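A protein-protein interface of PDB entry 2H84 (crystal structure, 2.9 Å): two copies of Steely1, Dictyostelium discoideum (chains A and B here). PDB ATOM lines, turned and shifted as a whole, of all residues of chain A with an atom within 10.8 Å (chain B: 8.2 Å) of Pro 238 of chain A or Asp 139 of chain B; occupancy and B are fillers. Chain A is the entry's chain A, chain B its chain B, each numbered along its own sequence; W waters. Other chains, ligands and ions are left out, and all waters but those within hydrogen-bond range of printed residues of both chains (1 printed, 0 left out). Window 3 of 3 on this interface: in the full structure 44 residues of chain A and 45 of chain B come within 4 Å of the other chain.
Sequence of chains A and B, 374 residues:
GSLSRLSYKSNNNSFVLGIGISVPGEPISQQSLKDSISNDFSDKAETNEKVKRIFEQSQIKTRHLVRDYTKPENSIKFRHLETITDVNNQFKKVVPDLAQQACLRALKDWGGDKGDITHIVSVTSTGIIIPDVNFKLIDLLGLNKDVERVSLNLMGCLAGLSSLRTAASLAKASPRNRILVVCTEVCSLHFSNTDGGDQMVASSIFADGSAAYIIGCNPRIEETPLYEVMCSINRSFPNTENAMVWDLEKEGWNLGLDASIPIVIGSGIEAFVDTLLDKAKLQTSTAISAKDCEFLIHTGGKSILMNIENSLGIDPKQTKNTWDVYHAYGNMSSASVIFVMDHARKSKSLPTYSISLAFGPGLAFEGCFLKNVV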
ATOM      1  N   ASN A 234       8.599  -5.432  18.641  1.00  0.00           N
ATOM      2  CA  ASN A 234       8.927  -5.267  20.056  1.00  0.00           C
ATOM      3  C   ASN A 234       7.680  -5.466  20.896  1.00  0.00           C
ATOM      4  O   ASN A 234       6.560  -5.244  20.435  1.00  0.00           O
ATOM      5  CB  ASN A 234       9.588  -3.901  20.361  1.00  0.00           C
ATOM      6  CG  ASN A 234       8.641  -2.715  20.233  1.00  0.00           C
ATOM      7  OD1 ASN A 234       9.031  -1.584  20.499  1.00  0.00           O
ATOM      8  ND2 ASN A 234       7.404  -2.966  19.824  1.00  0.00           N
ATOM      9  N   ARG A 235       7.870  -5.908  22.131  1.00  0.00           N
ATOM     10  CA  ARG A 235       6.739  -6.158  23.017  1.00  0.00           C
ATOM     11  C   ARG A 235       7.001  -5.553  24.385  1.00  0.00           C
ATOM     12  O   ARG A 235       8.146  -5.501  24.842  1.00  0.00           O
ATOM     13  CB  ARG A 235       6.516  -7.673  23.167  1.00  0.00           C
ATOM     14  CG  ARG A 235       5.275  -8.082  23.968  1.00  0.00           C
ATOM     15  CD  ARG A 235       4.205  -8.657  23.055  1.00  0.00           C
ATOM     16  NE  ARG A 235       4.534 -10.002  22.602  1.00  0.00           N
ATOM     17  CZ  ARG A 235       4.003 -10.586  21.532  1.00  0.00           C
ATOM     18  NH1 ARG A 235       3.116  -9.947  20.782  1.00  0.00           N
ATOM     19  NH2 ARG A 235       4.342 -11.828  21.226  1.00  0.00           N
ATOM     20  N   SER A 236       5.938  -5.095  25.039  1.00  0.00           N
ATOM     21  CA  SER A 236       6.065  -4.532  26.372  1.00  0.00           C
ATOM     22  C   SER A 236       5.233  -5.384  27.323  1.00  0.00           C
ATOM     23  O   SER A 236       4.188  -5.916  26.935  1.00  0.00           O
ATOM     24  CB  SER A 236       5.572  -3.090  26.404  1.00  0.00           C
ATOM     25  OG  SER A 236       4.173  -3.026  26.244  1.00  0.00           O
ATOM     26  N   PHE A 237       5.704  -5.534  28.557  1.00  0.00           N
ATOM     27  CA  PHE A 237       4.977  -6.322  29.547  1.00  0.00           C
ATOM     28  C   PHE A 237       4.606  -5.494  30.781  1.00  0.00           C
ATOM     29  O   PHE A 237       5.470  -5.002  31.514  1.00  0.00           O
ATOM     30  CB  PHE A 237       5.794  -7.549  29.979  1.00  0.00           C
ATOM     31  CG  PHE A 237       6.170  -8.463  28.840  1.00  0.00           C
ATOM     32  CD1 PHE A 237       7.319  -8.221  28.089  1.00  0.00           C
ATOM     33  CD2 PHE A 237       5.365  -9.561  28.513  1.00  0.00           C
ATOM     34  CE1 PHE A 237       7.650  -9.043  27.020  1.00  0.00           C
ATOM     35  CE2 PHE A 237       5.686 -10.384  27.452  1.00  0.00           C
ATOM     36  CZ  PHE A 237       6.832 -10.133  26.706  1.00  0.00           C
ATOM     37  N   PRO A 238       3.303  -5.328  31.023  1.00  0.00           N
ATOM     38  CA  PRO A 238       2.809  -4.558  32.168  1.00  0.00           C
ATOM     39  C   PRO A 238       3.214  -5.127  33.518  1.00  0.00           C
ATOM     40  O   PRO A 238       3.562  -6.298  33.628  1.00  0.00           O
ATOM     41  CB  PRO A 238       1.299  -4.588  31.973  1.00  0.00           C
ATOM     42  CG  PRO A 238       1.161  -4.646  30.499  1.00  0.00           C
ATOM     43  CD  PRO A 238       2.200  -5.661  30.111  1.00  0.00           C
ATOM     44  N   ASN A 239       3.181  -4.272  34.538  1.00  0.00           N
ATOM     45  CA  ASN A 239       3.502  -4.654  35.908  1.00  0.00           C
ATOM     46  C   ASN A 239       4.859  -5.339  36.079  1.00  0.00           C
ATOM     47  O   ASN A 239       4.953  -6.339  36.782  1.00  0.00           O
ATOM     48  CB  ASN A 239       2.399  -5.572  36.456  1.00  0.00           C
ATOM     49  CG  ASN A 239       1.005  -5.107  36.078  1.00  0.00           C
ATOM     50  OD1 ASN A 239       0.522  -4.091  36.507  1.00  0.00           O
ATOM     51  ND2 ASN A 239       0.367  -5.865  35.266  1.00  0.00           N
ATOM     52  N   THR A 240       5.906  -4.815  35.446  1.00  0.00           N
ATOM     53  CA  THR A 240       7.241  -5.417  35.573  1.00  0.00           C
ATOM     54  C   THR A 240       8.334  -4.362  35.487  1.00  0.00           C
ATOM     55  O   THR A 240       9.510  -4.678  35.271  1.00  0.00           O
ATOM     56  CB  THR A 240       7.526  -6.470  34.460  1.00  0.00           C
ATOM     57  OG1 THR A 240       7.371  -5.862  33.171  1.00  0.00           O
ATOM     58  CG2 THR A 240       6.603  -7.659  34.582  1.00  0.00           C
ATOM     59  N   GLU A 241       7.949  -3.105  35.657  1.00  0.00           N
ATOM     60  CA  GLU A 241       8.915  -2.038  35.554  1.00  0.00           C
ATOM     61  C   GLU A 241      10.070  -2.194  36.535  1.00  0.00           C
ATOM     62  O   GLU A 241      11.176  -1.715  36.270  1.00  0.00           O
ATOM     63  CB  GLU A 241       8.220  -0.689  35.713  1.00  0.00           C
ATOM     64  CG  GLU A 241       7.307  -0.391  34.541  1.00  0.00           C
ATOM     65  CD  GLU A 241       6.671   0.987  34.604  1.00  0.00           C
ATOM     66  OE1 GLU A 241       5.917   1.333  33.668  1.00  0.00           O
ATOM     67  OE2 GLU A 241       6.921   1.722  35.582  1.00  0.00           O
ATOM     68  N   ASN A 242       9.839  -2.891  37.644  1.00  0.00           N
ATOM     69  CA  ASN A 242      10.891  -3.078  38.634  1.00  0.00           C
ATOM     70  C   ASN A 242      11.779  -4.299  38.435  1.00  0.00           C
ATOM     71  O   ASN A 242      12.693  -4.524  39.219  1.00  0.00           O
ATOM     72  CB  ASN A 242      10.308  -3.140  40.034  1.00  0.00           C
ATOM     73  CG  ASN A 242       9.570  -1.883  40.417  1.00  0.00           C
ATOM     74  OD1 ASN A 242       9.981  -0.763  40.110  1.00  0.00           O
ATOM     75  ND2 ASN A 242       8.463  -2.066  41.109  1.00  0.00           N
ATOM     76  N   ALA A 243      11.512  -5.076  37.389  1.00  0.00           N
ATOM     77  CA  ALA A 243      12.305  -6.261  37.086  1.00  0.00           C
ATOM     78  C   ALA A 243      13.771  -5.882  36.918  1.00  0.00           C
ATOM     79  O   ALA A 243      14.670  -6.585  37.379  1.00  0.00           O
ATOM     80  CB  ALA A 243      11.804  -6.891  35.841  1.00  0.00           C
ATOM     81  N   SER A 260      13.395 -13.227  38.841  1.00  0.00           N
ATOM     82  CA  SER A 260      12.363 -13.728  37.944  1.00  0.00           C
ATOM     83  C   SER A 260      12.642 -13.448  36.466  1.00  0.00           C
ATOM     84  O   SER A 260      12.057 -14.066  35.575  1.00  0.00           O
ATOM     85  CB  SER A 260      11.017 -13.113  38.314  1.00  0.00           C
ATOM     86  OG  SER A 260      11.044 -11.723  38.058  1.00  0.00           O
ATOM     87  N   VAL A 264      10.715 -15.158  33.379  1.00  0.00           N
ATOM     88  CA  VAL A 264       9.727 -14.286  32.768  1.00  0.00           C
ATOM     89  C   VAL A 264      10.051 -14.250  31.280  1.00  0.00           C
ATOM     90  O   VAL A 264       9.166 -14.076  30.450  1.00  0.00           O
ATOM     91  CB  VAL A 264       9.785 -12.832  33.309  1.00  0.00           C
ATOM     92  CG1 VAL A 264       8.712 -11.966  32.645  1.00  0.00           C
ATOM     93  CG2 VAL A 264       9.601 -12.816  34.798  1.00  0.00           C
ATOM     94  N   GLY A 360      15.087  -6.008  27.691  1.00  0.00           N
ATOM     95  CA  GLY A 360      15.619  -5.027  28.622  1.00  0.00           C
ATOM     96  C   GLY A 360      14.580  -4.400  29.505  1.00  0.00           C
ATOM     97  O   GLY A 360      13.473  -4.895  29.632  1.00  0.00           O
ATOM     98  N   PRO A 361      14.967  -3.313  30.181  1.00  0.00           N
ATOM     99  CA  PRO A 361      14.062  -2.587  31.079  1.00  0.00           C
ATOM    100  C   PRO A 361      12.612  -2.372  30.546  1.00  0.00           C
ATOM    101  O   PRO A 361      12.486  -2.041  29.336  1.00  0.00           O
ATOM    102  CB  PRO A 361      14.814  -1.301  31.280  1.00  0.00           C
ATOM    103  CG  PRO A 361      16.222  -1.933  31.622  1.00  0.00           C
ATOM    104  CD  PRO A 361      16.386  -3.061  30.578  1.00  0.00           C
ATOM    105  N   GLY A 362      11.627  -2.512  31.406  1.00  0.00           N
ATOM    106  CA  GLY A 362      10.376  -2.376  31.006  1.00  0.00           C
ATOM    107  C   GLY A 362       9.442  -3.332  31.753  1.00  0.00           C
ATOM    108  O   GLY A 362       8.544  -2.715  32.469  1.00  0.00           O
ATOM    109  N   LEU A 363       9.418  -4.646  31.598  1.00  0.00           N
ATOM    110  CA  LEU A 363      10.242  -5.236  30.692  1.00  0.00           C
ATOM    111  C   LEU A 363       9.869  -5.115  29.215  1.00  0.00           C
ATOM    112  O   LEU A 363       8.705  -4.809  28.817  1.00  0.00           O
ATOM    113  CB  LEU A 363      10.307  -6.684  31.094  1.00  0.00           C
ATOM    114  CG  LEU A 363      10.867  -6.924  32.492  1.00  0.00           C
ATOM    115  CD1 LEU A 363      10.437  -8.233  33.162  1.00  0.00           C
ATOM    116  CD2 LEU A 363      12.363  -6.900  32.309  1.00  0.00           C
ATOM    117  N   ALA A 364      10.769  -5.485  28.310  1.00  0.00           N
ATOM    118  CA  ALA A 364      10.487  -5.436  26.857  1.00  0.00           C
ATOM    119  C   ALA A 364      11.299  -6.359  26.008  1.00  0.00           C
ATOM    120  O   ALA A 364      12.439  -6.606  26.302  1.00  0.00           O
ATOM    121  CB  ALA A 364      10.577  -3.957  26.389  1.00  0.00           C
ATOM    122  N   PHE A 365      10.681  -6.859  24.949  1.00  0.00           N
ATOM    123  CA  PHE A 365      11.404  -7.753  24.059  1.00  0.00           C
ATOM    124  C   PHE A 365      11.591  -7.016  22.765  1.00  0.00           C
ATOM    125  O   PHE A 365      10.747  -6.211  22.379  1.00  0.00           O
ATOM    126  CB  PHE A 365      10.624  -9.047  23.767  1.00  0.00           C
ATOM    127  CG  PHE A 365      10.408  -9.935  24.972  1.00  0.00           C
ATOM    128  CD1 PHE A 365       9.623 -11.084  24.857  1.00  0.00           C
ATOM    129  CD2 PHE A 365      10.979  -9.634  26.211  1.00  0.00           C
ATOM    130  CE1 PHE A 365       9.410 -11.929  25.952  1.00  0.00           C
ATOM    131  CE2 PHE A 365      10.771 -10.471  27.318  1.00  0.00           C
ATOM    132  CZ  PHE A 365       9.981 -11.622  27.187  1.00  0.00           C
ATOM    133  N   GLN B 100       1.623  12.145  30.220  1.00  0.00           N
ATOM    134  CA  GLN B 100       0.368  11.425  30.014  1.00  0.00           C
ATOM    135  C   GLN B 100      -0.703  12.450  29.628  1.00  0.00           C
ATOM    136  O   GLN B 100      -1.523  12.234  28.737  1.00  0.00           O
ATOM    137  CB  GLN B 100      -0.044  10.686  31.300  1.00  0.00           C
ATOM    138  CG  GLN B 100      -1.187   9.678  31.056  1.00  0.00           C
ATOM    139  CD  GLN B 100      -1.704   9.070  32.333  1.00  0.00           C
ATOM    140  OE1 GLN B 100      -2.696   8.322  32.326  1.00  0.00           O
ATOM    141  NE2 GLN B 100      -1.030   9.383  33.431  1.00  0.00           N
ATOM    142  N   LYS B 114      -6.560   5.236  19.521  1.00  0.00           N
ATOM    143  CA  LYS B 114      -5.261   4.955  20.127  1.00  0.00           C
ATOM    144  C   LYS B 114      -4.706   3.543  19.904  1.00  0.00           C
ATOM    145  O   LYS B 114      -3.645   3.229  20.423  1.00  0.00           O
ATOM    146  CB  LYS B 114      -5.354   5.204  21.641  1.00  0.00           C
ATOM    147  CG  LYS B 114      -5.922   4.032  22.423  1.00  0.00           C
ATOM    148  CD  LYS B 114      -6.272   4.447  23.825  1.00  0.00           C
ATOM    149  CE  LYS B 114      -6.844   3.284  24.605  1.00  0.00           C
ATOM    150  NZ  LYS B 114      -7.511   3.735  25.857  1.00  0.00           N
ATOM    151  N   VAL B 133      10.058   7.105  29.576  1.00  0.00           N
ATOM    152  CA  VAL B 133       8.695   7.609  29.536  1.00  0.00           C
ATOM    153  C   VAL B 133       7.793   6.935  28.501  1.00  0.00           C
ATOM    154  O   VAL B 133       6.623   6.679  28.778  1.00  0.00           O
ATOM    155  CB  VAL B 133       8.674   9.132  29.273  1.00  0.00           C
ATOM    156  CG1 VAL B 133       7.312   9.712  29.630  1.00  0.00           C
ATOM    157  CG2 VAL B 133       9.753   9.807  30.077  1.00  0.00           C
ATOM    158  N   ASN B 134       8.320   6.646  27.313  1.00  0.00           N
ATOM    159  CA  ASN B 134       7.498   6.025  26.284  1.00  0.00           C
ATOM    160  C   ASN B 134       6.976   4.641  26.675  1.00  0.00           C
ATOM    161  O   ASN B 134       5.890   4.235  26.246  1.00  0.00           O
ATOM    162  CB  ASN B 134       8.246   5.966  24.941  1.00  0.00           C
ATOM    163  CG  ASN B 134       9.556   5.237  25.026  1.00  0.00           C
ATOM    164  OD1 ASN B 134       9.664   4.088  24.697  1.00  0.00           O
ATOM    165  ND2 ASN B 134      10.552   5.909  25.475  1.00  0.00           N
ATOM    166  N   PHE B 135       7.727   3.918  27.500  1.00  0.00           N
ATOM    167  CA  PHE B 135       7.288   2.592  27.939  1.00  0.00           C
ATOM    168  C   PHE B 135       6.180   2.742  28.977  1.00  0.00           C
ATOM    169  O   PHE B 135       5.141   2.087  28.893  1.00  0.00           O
ATOM    170  CB  PHE B 135       8.451   1.811  28.560  1.00  0.00           C
ATOM    171  CG  PHE B 135       8.049   0.479  29.120  1.00  0.00           C
ATOM    172  CD1 PHE B 135       8.093  -0.666  28.327  1.00  0.00           C
ATOM    173  CD2 PHE B 135       7.558   0.375  30.418  1.00  0.00           C
ATOM    174  CE1 PHE B 135       7.660  -1.886  28.814  1.00  0.00           C
ATOM    175  CE2 PHE B 135       7.123  -0.837  30.911  1.00  0.00           C
ATOM    176  CZ  PHE B 135       7.172  -1.973  30.103  1.00  0.00           C
ATOM    177  N   LYS B 136       6.425   3.602  29.958  1.00  0.00           N
ATOM    178  CA  LYS B 136       5.468   3.855  31.027  1.00  0.00           C
ATOM    179  C   LYS B 136       4.088   4.278  30.521  1.00  0.00           C
ATOM    180  O   LYS B 136       3.065   4.000  31.156  1.00  0.00           O
ATOM    181  CB  LYS B 136       6.021   4.934  31.962  1.00  0.00           C
ATOM    182  CG  LYS B 136       6.922   4.413  33.060  1.00  0.00           C
ATOM    183  CD  LYS B 136       7.561   5.550  33.829  1.00  0.00           C
ATOM    184  CE  LYS B 136       7.867   5.147  35.255  1.00  0.00           C
ATOM    185  NZ  LYS B 136       8.472   3.796  35.315  1.00  0.00           N
ATOM    186  N   LEU B 137       4.072   4.954  29.378  1.00  0.00           N
ATOM    187  CA  LEU B 137       2.833   5.445  28.792  1.00  0.00           C
ATOM    188  C   LEU B 137       2.047   4.349  28.085  1.00  0.00           C
ATOM    189  O   LEU B 137       0.824   4.434  27.980  1.00  0.00           O
ATOM    190  CB  LEU B 137       3.133   6.593  27.813  1.00  0.00           C
ATOM    191  CG  LEU B 137       3.515   7.956  28.414  1.00  0.00           C
ATOM    192  CD1 LEU B 137       4.166   8.855  27.354  1.00  0.00           C
ATOM    193  CD2 LEU B 137       2.268   8.610  28.999  1.00  0.00           C
ATOM    194  N   ILE B 138       2.740   3.322  27.600  1.00  0.00           N
ATOM    195  CA  ILE B 138       2.051   2.248  26.897  1.00  0.00           C
ATOM    196  C   ILE B 138       0.856   1.797  27.708  1.00  0.00           C
ATOM    197  O   ILE B 138      -0.274   1.772  27.215  1.00  0.00           O
ATOM    198  CB  ILE B 138       2.966   1.027  26.644  1.00  0.00           C
ATOM    199  CG1 ILE B 138       4.060   1.400  25.640  1.00  0.00           C
ATOM    200  CG2 ILE B 138       2.131  -0.148  26.139  1.00  0.00           C
ATOM    201  CD1 ILE B 138       4.949   0.258  25.243  1.00  0.00           C
ATOM    202  N   ASP B 139       1.117   1.469  28.968  1.00  0.00           N
ATOM    203  CA  ASP B 139       0.082   0.998  29.876  1.00  0.00           C
ATOM    204  C   ASP B 139      -0.827   2.123  30.366  1.00  0.00           C
ATOM    205  O   ASP B 139      -2.022   1.905  30.556  1.00  0.00           O
ATOM    206  CB  ASP B 139       0.724   0.304  31.074  1.00  0.00           C
ATOM    207  CG  ASP B 139      -0.194  -0.715  31.723  1.00  0.00           C
ATOM    208  OD1 ASP B 139      -0.619  -1.661  31.017  1.00  0.00           O
ATOM    209  OD2 ASP B 139      -0.479  -0.566  32.933  1.00  0.00           O
ATOM    210  N   LEU B 140      -0.258   3.311  30.577  1.00  0.00           N
ATOM    211  CA  LEU B 140      -1.025   4.468  31.047  1.00  0.00           C
ATOM    212  C   LEU B 140      -2.100   4.861  30.042  1.00  0.00           C
ATOM    213  O   LEU B 140      -3.262   5.061  30.402  1.00  0.00           O
ATOM    214  CB  LEU B 140      -0.110   5.670  31.295  1.00  0.00           C
ATOM    215  CG  LEU B 140       0.803   5.589  32.515  1.00  0.00           C
ATOM    216  CD1 LEU B 140       1.781   6.737  32.503  1.00  0.00           C
ATOM    217  CD2 LEU B 140      -0.035   5.635  33.771  1.00  0.00           C
ATOM    218  N   LEU B 141      -1.711   4.960  28.778  1.00  0.00           N
ATOM    219  CA  LEU B 141      -2.638   5.336  27.725  1.00  0.00           C
ATOM    220  C   LEU B 141      -3.382   4.122  27.187  1.00  0.00           C
ATOM    221  O   LEU B 141      -4.383   4.258  26.494  1.00  0.00           O
ATOM    222  CB  LEU B 141      -1.875   6.018  26.585  1.00  0.00           C
ATOM    223  CG  LEU B 141      -1.031   7.248  26.950  1.00  0.00           C
ATOM    224  CD1 LEU B 141      -0.265   7.735  25.716  1.00  0.00           C
ATOM    225  CD2 LEU B 141      -1.933   8.350  27.502  1.00  0.00           C
ATOM    226  N   GLY B 142      -2.895   2.930  27.509  1.00  0.00           N
ATOM    227  CA  GLY B 142      -3.549   1.731  27.020  1.00  0.00           C
ATOM    228  C   GLY B 142      -3.323   1.555  25.530  1.00  0.00           C
ATOM    229  O   GLY B 142      -4.244   1.232  24.777  1.00  0.00           O
ATOM    230  N   LEU B 143      -2.088   1.777  25.096  1.00  0.00           N
ATOM    231  CA  LEU B 143      -1.754   1.629  23.695  1.00  0.00           C
ATOM    232  C   LEU B 143      -1.425   0.168  23.452  1.00  0.00           C
ATOM    233  O   LEU B 143      -1.305  -0.617  24.389  1.00  0.00           O
ATOM    234  CB  LEU B 143      -0.551   2.490  23.366  1.00  0.00           C
ATOM    235  CG  LEU B 143      -0.661   3.928  23.861  1.00  0.00           C
ATOM    236  CD1 LEU B 143       0.682   4.607  23.652  1.00  0.00           C
ATOM    237  CD2 LEU B 143      -1.774   4.670  23.129  1.00  0.00           C
ATOM    238  N   ASN B 144      -1.291  -0.200  22.190  1.00  0.00           N
ATOM    239  CA  ASN B 144      -0.958  -1.570  21.852  1.00  0.00           C
ATOM    240  C   ASN B 144       0.361  -1.936  22.543  1.00  0.00           C
ATOM    241  O   ASN B 144       1.370  -1.244  22.388  1.00  0.00           O
ATOM    242  CB  ASN B 144      -0.827  -1.692  20.331  1.00  0.00           C
ATOM    243  CG  ASN B 144      -0.608  -3.122  19.863  1.00  0.00           C
ATOM    244  OD1 ASN B 144      -1.236  -3.569  18.900  1.00  0.00           O
ATOM    245  ND2 ASN B 144       0.293  -3.841  20.525  1.00  0.00           N
ATOM    246  N   LYS B 145       0.349  -3.020  23.307  1.00  0.00           N
ATOM    247  CA  LYS B 145       1.551  -3.478  24.007  1.00  0.00           C
ATOM    248  C   LYS B 145       2.750  -3.630  23.050  1.00  0.00           C
ATOM    249  O   LYS B 145       3.903  -3.570  23.471  1.00  0.00           O
ATOM    250  CB  LYS B 145       1.281  -4.831  24.665  1.00  0.00           C
ATOM    251  CG  LYS B 145       0.965  -5.895  23.615  1.00  0.00           C
ATOM    252  CD  LYS B 145       0.820  -7.297  24.172  1.00  0.00           C
ATOM    253  CE  LYS B 145       0.388  -8.243  23.058  1.00  0.00           C
ATOM    254  NZ  LYS B 145       0.223  -9.649  23.537  1.00  0.00           N
ATOM    255  N   VAL B 147       3.282  -1.611  20.428  1.00  0.00           N
ATOM    256  CA  VAL B 147       3.626  -0.337  19.801  1.00  0.00           C
ATOM    257  C   VAL B 147       5.140  -0.178  19.832  1.00  0.00           C
ATOM    258  O   VAL B 147       5.779  -0.549  20.809  1.00  0.00           O
ATOM    259  CB  VAL B 147       2.935   0.862  20.528  1.00  0.00           C
ATOM    260  CG1 VAL B 147       3.462   1.008  21.940  1.00  0.00           C
ATOM    261  CG2 VAL B 147       3.145   2.136  19.742  1.00  0.00           C
HETATM  262  O   HOH W   1       3.775   3.516  34.305  1.00  0.00           O
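The backbone carbonyl oxygen (O) of Arg 235 of chain A lies within hydrogen-bond range of the backbone NH (N) of Phe 365 of chain A (2.9 Å).
The backbone carbonyl oxygen (O) of Leu 363 of chain A is in hydrogen-bond range of the backbone NH (N) of Phe 237 of chain A (3.1 Å).
OG1 of Thr 240 of chain A is in hydrogen-bond range of O of Gly 362 of chain A, 3.4 Å away.
N of Leu 363 of chain A is in hydrogen-bond range of OG1 of Thr 240 of chain A, at 2.9 Å.
The backbone NH (N) of Glu 241 of chain A lies close to the backbone carbonyl oxygen (O) of Gly 362 of chain A, at 3.3 Å.
O of Ile 138 of chain B lies within hydrogen-bond range of N of Leu 143 of chain B (2.8 Å).
The side-chain amide nitrogen of Asn 234 of chain A is in hydrogen-bond range of the backbone carbonyl oxygen of Val 147 of chain B, at 3.1 Å.
O of Lys 145 of chain B lies within hydrogen-bond range of OG of Ser 236 of chain A, 2.8 Å away.
OE2 of Glu 241 of chain A is in salt-bridge range of NZ of Lys 136 of chain B, 2.6 Å away.
Of the 16 printed residues of chain B, 6 touch a printed residue of chain A.
Printed residues of chain B that touch a printed residue of chain A: Phe 135, Lys 136, Ile 138, Asp 139, Lys 145 and Val 147.
Hydrophobic or aromatic side chains of chain B that line the printed part of chain A: Phe 135 and Ile 138.
Of the 18 printed residues of chain A, 8 touch a printed residue of chain B.
Among the printed residues, 11 pairs touch across the chains.
Among the printed residues, Asp or Glu carboxylates within 4 Å of a Lys or Arg side-chain nitrogen of the other chain: Glu 241 of chain A with Lys 136 of chain B (2.6 Å).
Among the printed residues, pairs that only touch across the chains: Gly 362 of chain A with Phe 135 of chain B (2.8 Å), Leu 363 of chain A with Phe 135 of chain B (3.1 Å), Ser 236 of chain A with Phe 135 of chain B (3.4 Å), Pro 238 of chain A with Asp 139 of chain B (3.5 Å), Ser 236 of chain A with Ile 138 of chain B (3.5 Å), Glu 241 of chain A with Phe 135 of chain B (3.7 Å), Phe 237 of chain A with Phe 135 of chain B (3.8 Å) and Arg 235 of chain A with Lys 145 of chain B (3.8 Å).
Water W1 bridges OE1 of Glu 241 of chain A (3.1 Å) and O of Lys 136 of chain B (3.3 Å).
Pro 238 of chain A touches just one residue of chain B: Asp 139 (3.5 Å).
Asp 139 of chain B touches one residue of chain A.
Ile 138 of chain B touches just one residue of chain A: Ser 236 (3.5 Å).
Leu 140 of chain B touches none of the printed residues of chain A.
Of the printed residues of chain B, Glu 241 of chain A touches Phe 135 (3.7 Å) and Lys 136 (2.6 Å).
Of the printed residues of chain B, Gly 362 of chain A touches Phe 135.
Printed residues of chain B within 4 Å of Leu 363 of chain A: Phe 135.
Printed residues of chain A within 4 Å of Val 147 of chain B: Asn 234.
Val 133 of chain B touches none of the printed residues of chain A.
The nearest residue of chain B that does not touch Pro 238 of chain A is Phe 135 of chain B (5.2 Å).
The nearest printed residue of chain A that does not touch Phe 135 of chain B is Ala 364 of chain A (4.3 Å).
No position is printed for both chains.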
